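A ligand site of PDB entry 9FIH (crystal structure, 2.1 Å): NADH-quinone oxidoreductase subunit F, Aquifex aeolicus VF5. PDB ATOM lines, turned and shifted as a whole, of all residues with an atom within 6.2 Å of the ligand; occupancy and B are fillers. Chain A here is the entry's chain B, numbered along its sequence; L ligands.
N of Cys 350 lies close to S1 of the ligand.
SG of Cys 350 binds FE2 of the ligand (2.2 Å).
S2 of the ligand lies close to N of Cys 347 (3.7 Å).
SG of Cys 347 is bound to FE3 of the ligand (2.3 Å).
The side-chain sulfur (SG) of Cys 353 is bound to an iron atom (FE4) of the ligand (2.3 Å).
The side-chain sulfur of Cys 393 binds an iron atom (FE1) of the ligand (2.3 Å).
N of Gln 349 sits close to S1 of the ligand (3.3 Å).
The side-chain amide oxygen (OE1) of Gln 349 sits close to a sulfur (S4) of the ligand (3.6 Å).
S3 of the ligand lies close to N of Gly 396, 3.4 Å away.
A sulfur (S1) of the ligand sits close to the backbone NH (N) of Gly 348, 3.5 Å away.
N of Ile 392 lies close to SG of Cys 350, at 3.7 Å.
OG1 of Thr 346 sits close to SG of Cys 353 (3.2 Å).
O of Cys 353 sits close to SG of Cys 357, 3.4 Å away.
O of Ile 387 lies within hydrogen-bond range of N of Cys 353, at 3.5 Å.
The side-chain sulfur of Cys 393 lies close to the backbone NH of Leu 395 (3.5 Å).
The backbone carbonyl oxygen of Pro 199 sits close to the side-chain amide oxygen of Gln 349, 2.9 Å away.
The backbone NH (N) of Gly 348 lies close to the side-chain hydroxyl (OG1) of Thr 346, 3.4 Å away.
O of Gly 348 is in hydrogen-bond range of NH1 of Arg 354, at 2.8 Å.
Ile 181 touches the ligand.
Pro 199 touches the ligand.
Thr 346 touches the ligand.
CB of Ser 391 touches S3 of the ligand (3.6 Å).
CG1 of Ile 392 touches S4 of the ligand, 3.5 Å away.
Leu 395 touches the ligand (CB to S2, 3.7 Å).
Hydrophobic or aromatic side chains within 4 Å of the ligand: Ile 181, Pro 199, Ile 392 and Leu 395.
Within 4 Å of the ligand: Ile 181, Pro 199, Thr 346, Cys 347, Gly 348, Gln 349, Cys 350, Cys 353, Ser 391, Ile 392, Cys 393, Leu 395 and Gly 396.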
ATOM      1  N   ILE A 181       7.057  11.417 -19.944  1.00  0.00           N
ATOM      2  CA  ILE A 181       5.924  10.904 -19.189  1.00  0.00           C
ATOM      3  C   ILE A 181       4.608  11.405 -19.794  1.00  0.00           C
ATOM      4  O   ILE A 181       3.569  10.762 -19.597  1.00  0.00           O
ATOM      5  CB  ILE A 181       6.032  11.300 -17.701  1.00  0.00           C
ATOM      6  CG1 ILE A 181       5.080  10.532 -16.844  1.00  0.00           C
ATOM      7  CG2 ILE A 181       5.854  12.805 -17.481  1.00  0.00           C
ATOM      8  CD1 ILE A 181       5.213   9.032 -16.946  1.00  0.00           C
ATOM      9  N   HIS A 198       1.340  14.474 -14.797  1.00  0.00           N
ATOM     10  CA  HIS A 198       1.307  13.508 -13.708  1.00  0.00           C
ATOM     11  C   HIS A 198       0.296  12.403 -14.013  1.00  0.00           C
ATOM     12  O   HIS A 198      -0.902  12.664 -14.039  1.00  0.00           O
ATOM     13  CB  HIS A 198       0.965  14.181 -12.380  1.00  0.00           C
ATOM     14  CG  HIS A 198       2.092  14.955 -11.797  1.00  0.00           C
ATOM     15  ND1 HIS A 198       1.906  15.880 -10.810  1.00  0.00           N
ATOM     16  CD2 HIS A 198       3.411  14.934 -12.033  1.00  0.00           C
ATOM     17  CE1 HIS A 198       3.080  16.411 -10.478  1.00  0.00           C
ATOM     18  NE2 HIS A 198       4.011  15.839 -11.206  1.00  0.00           N
ATOM     19  N   PRO A 199       0.747  11.145 -14.218  1.00  0.00           N
ATOM     20  CA  PRO A 199      -0.185  10.034 -14.414  1.00  0.00           C
ATOM     21  C   PRO A 199      -1.191   9.896 -13.279  1.00  0.00           C
ATOM     22  O   PRO A 199      -0.907  10.240 -12.133  1.00  0.00           O
ATOM     23  CB  PRO A 199       0.744   8.811 -14.517  1.00  0.00           C
ATOM     24  CG  PRO A 199       2.034   9.376 -15.067  1.00  0.00           C
ATOM     25  CD  PRO A 199       2.143  10.725 -14.350  1.00  0.00           C
ATOM     26  N   ARG A 200      -2.363   9.352 -13.632  1.00  0.00           N
ATOM     27  CA  ARG A 200      -3.430   9.090 -12.685  1.00  0.00           C
ATOM     28  C   ARG A 200      -3.530   7.576 -12.444  1.00  0.00           C
ATOM     29  O   ARG A 200      -3.327   6.790 -13.358  1.00  0.00           O
ATOM     30  CB  ARG A 200      -4.782   9.533 -13.241  1.00  0.00           C
ATOM     31  CG  ARG A 200      -4.909  10.978 -13.685  1.00  0.00           C
ATOM     32  CD  ARG A 200      -6.208  11.157 -14.473  1.00  0.00           C
ATOM     33  NE  ARG A 200      -6.508  12.520 -14.946  1.00  0.00           N
ATOM     34  CZ  ARG A 200      -7.566  12.821 -15.707  1.00  0.00           C
ATOM     35  NH1 ARG A 200      -8.365  11.853 -16.144  1.00  0.00           N
ATOM     36  NH2 ARG A 200      -7.840  14.073 -16.028  1.00  0.00           N
ATOM     37  N   GLU A 345      13.332  11.160 -16.555  1.00  0.00           N
ATOM     38  CA  GLU A 345      11.920  11.175 -16.922  1.00  0.00           C
ATOM     39  C   GLU A 345      10.936  10.806 -15.801  1.00  0.00           C
ATOM     40  O   GLU A 345       9.744  11.074 -15.950  1.00  0.00           O
ATOM     41  CB  GLU A 345      11.699  10.261 -18.136  1.00  0.00           C
ATOM     42  CG  GLU A 345      12.484  10.689 -19.368  1.00  0.00           C
ATOM     43  CD  GLU A 345      12.422  12.176 -19.693  1.00  0.00           C
ATOM     44  OE1 GLU A 345      11.340  12.824 -19.582  1.00  0.00           O
ATOM     45  OE2 GLU A 345      13.497  12.680 -20.093  1.00  0.00           O
ATOM     46  N   THR A 346      11.375  10.190 -14.692  1.00  0.00           N
ATOM     47  CA  THR A 346      10.432   9.897 -13.622  1.00  0.00           C
ATOM     48  C   THR A 346       9.711  11.201 -13.252  1.00  0.00           C
ATOM     49  O   THR A 346      10.348  12.245 -13.146  1.00  0.00           O
ATOM     50  CB  THR A 346      11.118   9.269 -12.410  1.00  0.00           C
ATOM     51  OG1 THR A 346      10.116   9.107 -11.407  1.00  0.00           O
ATOM     52  CG2 THR A 346      12.247  10.115 -11.840  1.00  0.00           C
ATOM     53  N   CYS A 347       8.395  11.154 -13.044  1.00  0.00           N
ATOM     54  CA  CYS A 347       7.652  12.352 -12.636  1.00  0.00           C
ATOM     55  C   CYS A 347       7.734  12.610 -11.128  1.00  0.00           C
ATOM     56  O   CYS A 347       7.389  13.706 -10.691  1.00  0.00           O
ATOM     57  CB  CYS A 347       6.218  12.308 -13.148  1.00  0.00           C
ATOM     58  SG  CYS A 347       5.060  11.327 -12.157  1.00  0.00           S
ATOM     59  N   GLY A 348       8.100  11.595 -10.335  1.00  0.00           N
ATOM     60  CA  GLY A 348       8.409  11.775  -8.923  1.00  0.00           C
ATOM     61  C   GLY A 348       7.221  11.588  -7.959  1.00  0.00           C
ATOM     62  O   GLY A 348       7.437  11.717  -6.752  1.00  0.00           O
ATOM     63  N   GLN A 349       6.025  11.249  -8.468  1.00  0.00           N
ATOM     64  CA  GLN A 349       4.823  11.085  -7.645  1.00  0.00           C
ATOM     65  C   GLN A 349       4.946   9.893  -6.693  1.00  0.00           C
ATOM     66  O   GLN A 349       4.458   9.948  -5.570  1.00  0.00           O
ATOM     67  CB  GLN A 349       3.555  10.762  -8.457  1.00  0.00           C
ATOM     68  CG  GLN A 349       2.866  11.955  -9.113  1.00  0.00           C
ATOM     69  CD  GLN A 349       1.571  11.569  -9.807  1.00  0.00           C
ATOM     70  OE1 GLN A 349       1.549  11.092 -10.960  1.00  0.00           O
ATOM     71  NE2 GLN A 349       0.460  11.774  -9.125  1.00  0.00           N
ATOM     72  N   CYS A 350       5.525   8.785  -7.189  1.00  0.00           N
ATOM     73  CA  CYS A 350       5.644   7.544  -6.427  1.00  0.00           C
ATOM     74  C   CYS A 350       7.057   7.443  -5.854  1.00  0.00           C
ATOM     75  O   CYS A 350       8.050   7.660  -6.544  1.00  0.00           O
ATOM     76  CB  CYS A 350       5.266   6.338  -7.279  1.00  0.00           C
ATOM     77  SG  CYS A 350       3.886   6.648  -8.424  1.00  0.00           S
ATOM     78  N   THR A 351       7.163   7.108  -4.560  1.00  0.00           N
ATOM     79  CA  THR A 351       8.434   7.249  -3.862  1.00  0.00           C
ATOM     80  C   THR A 351       9.453   6.267  -4.446  1.00  0.00           C
ATOM     81  O   THR A 351      10.527   6.676  -4.843  1.00  0.00           O
ATOM     82  CB  THR A 351       8.231   7.104  -2.362  1.00  0.00           C
ATOM     83  OG1 THR A 351       7.629   8.321  -1.918  1.00  0.00           O
ATOM     84  CG2 THR A 351       9.556   6.900  -1.629  1.00  0.00           C
ATOM     85  N   CYS A 353       9.708   4.852  -7.371  1.00  0.00           N
ATOM     86  CA  CYS A 353      10.056   5.303  -8.705  1.00  0.00           C
ATOM     87  C   CYS A 353      10.958   6.537  -8.651  1.00  0.00           C
ATOM     88  O   CYS A 353      11.993   6.562  -9.319  1.00  0.00           O
ATOM     89  CB  CYS A 353       8.809   5.609  -9.526  1.00  0.00           C
ATOM     90  SG  CYS A 353       9.151   6.110 -11.236  1.00  0.00           S
ATOM     91  N   ARG A 354      10.540   7.564  -7.884  1.00  0.00           N
ATOM     92  CA  ARG A 354      11.313   8.788  -7.737  1.00  0.00           C
ATOM     93  C   ARG A 354      12.750   8.493  -7.322  1.00  0.00           C
ATOM     94  O   ARG A 354      13.694   8.921  -7.992  1.00  0.00           O
ATOM     95  CB  ARG A 354      10.658   9.699  -6.703  1.00  0.00           C
ATOM     96  CG  ARG A 354      11.395  10.995  -6.391  1.00  0.00           C
ATOM     97  CD  ARG A 354      10.575  11.887  -5.481  1.00  0.00           C
ATOM     98  NE  ARG A 354      10.458  11.326  -4.130  1.00  0.00           N
ATOM     99  CZ  ARG A 354       9.378  10.807  -3.576  1.00  0.00           C
ATOM    100  NH1 ARG A 354       8.229  10.732  -4.266  1.00  0.00           N
ATOM    101  NH2 ARG A 354       9.457  10.382  -2.324  1.00  0.00           N
ATOM    102  N   CYS A 357      14.688   5.420  -9.655  1.00  0.00           N
ATOM    103  CA  CYS A 357      15.229   5.829 -10.958  1.00  0.00           C
ATOM    104  C   CYS A 357      16.500   6.645 -10.734  1.00  0.00           C
ATOM    105  O   CYS A 357      17.489   6.469 -11.448  1.00  0.00           O
ATOM    106  CB  CYS A 357      14.213   6.606 -11.796  1.00  0.00           C
ATOM    107  SG  CYS A 357      12.833   5.596 -12.430  1.00  0.00           S
ATOM    108  N   ILE A 387      12.066  -0.499  -7.956  1.00  0.00           N
ATOM    109  CA  ILE A 387      11.528   0.738  -8.496  1.00  0.00           C
ATOM    110  C   ILE A 387      10.009   0.608  -8.656  1.00  0.00           C
ATOM    111  O   ILE A 387       9.292   1.601  -8.518  1.00  0.00           O
ATOM    112  CB  ILE A 387      12.202   1.108  -9.829  1.00  0.00           C
ATOM    113  CG1 ILE A 387      13.721   1.152  -9.675  1.00  0.00           C
ATOM    114  CG2 ILE A 387      11.628   2.408 -10.397  1.00  0.00           C
ATOM    115  CD1 ILE A 387      14.489   1.378 -10.967  1.00  0.00           C
ATOM    116  N   THR A 390       4.351   0.198  -5.618  1.00  0.00           N
ATOM    117  CA  THR A 390       3.392   1.293  -5.404  1.00  0.00           C
ATOM    118  C   THR A 390       3.225   2.152  -6.649  1.00  0.00           C
ATOM    119  O   THR A 390       2.404   3.062  -6.643  1.00  0.00           O
ATOM    120  CB  THR A 390       3.756   2.157  -4.191  1.00  0.00           C
ATOM    121  OG1 THR A 390       4.758   3.109  -4.507  1.00  0.00           O
ATOM    122  CG2 THR A 390       4.161   1.318  -2.985  1.00  0.00           C
ATOM    123  N   SER A 391       3.970   1.843  -7.733  1.00  0.00           N
ATOM    124  CA  SER A 391       3.957   2.642  -8.950  1.00  0.00           C
ATOM    125  C   SER A 391       2.557   2.672  -9.553  1.00  0.00           C
ATOM    126  O   SER A 391       1.878   1.669  -9.602  1.00  0.00           O
ATOM    127  CB  SER A 391       4.969   2.151  -9.969  1.00  0.00           C
ATOM    128  OG  SER A 391       4.779   0.780 -10.317  1.00  0.00           O
ATOM    129  N   ILE A 392       2.131   3.843 -10.048  1.00  0.00           N
ATOM    130  CA  ILE A 392       0.806   3.986 -10.637  1.00  0.00           C
ATOM    131  C   ILE A 392       0.857   4.107 -12.161  1.00  0.00           C
ATOM    132  O   ILE A 392      -0.180   4.340 -12.771  1.00  0.00           O
ATOM    133  CB  ILE A 392       0.057   5.166 -10.014  1.00  0.00           C
ATOM    134  CG1 ILE A 392       0.762   6.505 -10.236  1.00  0.00           C
ATOM    135  CG2 ILE A 392      -0.206   4.914  -8.520  1.00  0.00           C
ATOM    136  CD1 ILE A 392       0.085   7.677  -9.544  1.00  0.00           C
ATOM    137  N   CYS A 393       2.049   4.008 -12.780  1.00  0.00           N
ATOM    138  CA  CYS A 393       2.150   4.000 -14.236  1.00  0.00           C
ATOM    139  C   CYS A 393       3.305   3.093 -14.663  1.00  0.00           C
ATOM    140  O   CYS A 393       4.070   2.604 -13.826  1.00  0.00           O
ATOM    141  CB  CYS A 393       2.265   5.401 -14.820  1.00  0.00           C
ATOM    142  SG  CYS A 393       3.948   5.980 -15.141  1.00  0.00           S
ATOM    143  N   GLY A 394       3.412   2.896 -15.981  1.00  0.00           N
ATOM    144  CA  GLY A 394       4.253   1.868 -16.574  1.00  0.00           C
ATOM    145  C   GLY A 394       5.732   2.217 -16.487  1.00  0.00           C
ATOM    146  O   GLY A 394       6.574   1.330 -16.620  1.00  0.00           O
ATOM    147  N   LEU A 395       6.072   3.500 -16.292  1.00  0.00           N
ATOM    148  CA  LEU A 395       7.471   3.888 -16.193  1.00  0.00           C
ATOM    149  C   LEU A 395       8.092   3.198 -14.979  1.00  0.00           C
ATOM    150  O   LEU A 395       9.121   2.525 -15.091  1.00  0.00           O
ATOM    151  CB  LEU A 395       7.577   5.401 -16.101  1.00  0.00           C
ATOM    152  CG  LEU A 395       8.983   5.992 -16.296  1.00  0.00           C
ATOM    153  CD1 LEU A 395       8.913   7.411 -16.799  1.00  0.00           C
ATOM    154  CD2 LEU A 395       9.821   5.944 -15.032  1.00  0.00           C
ATOM    155  N   GLY A 396       7.460   3.371 -13.807  1.00  0.00           N
ATOM    156  CA  GLY A 396       7.969   2.784 -12.589  1.00  0.00           C
ATOM    157  C   GLY A 396       8.036   1.270 -12.740  1.00  0.00           C
ATOM    158  O   GLY A 396       8.969   0.646 -12.250  1.00  0.00           O
ATOM    159  N   ALA A 397       7.071   0.704 -13.451  1.00  0.00           N
ATOM    160  CA  ALA A 397       6.974  -0.749 -13.557  1.00  0.00           C
ATOM    161  C   ALA A 397       8.095  -1.327 -14.428  1.00  0.00           C
ATOM    162  O   ALA A 397       8.448  -2.482 -14.246  1.00  0.00           O
ATOM    163  CB  ALA A 397       5.582  -1.135 -14.043  1.00  0.00           C
HETATM  164 FE1  LIG L   1       4.769   6.751 -13.158  1.00  0.00          FE
HETATM  165 FE2  LIG L   1       4.738   7.036 -10.467  1.00  0.00          FE
HETATM  166 FE3  LIG L   1       5.489   9.121 -12.025  1.00  0.00          FE
HETATM  167 FE4  LIG L   1       7.120   6.926 -11.777  1.00  0.00          FE
HETATM  168  S1  LIG L   1       6.527   8.439 -10.129  1.00  0.00           S
HETATM  169  S2  LIG L   1       6.605   8.022 -13.685  1.00  0.00           S
HETATM  170  S3  LIG L   1       5.556   5.236 -11.653  1.00  0.00           S
HETATM  171  S4  LIG L   1       3.399   8.130 -11.924  1.00  0.00           S
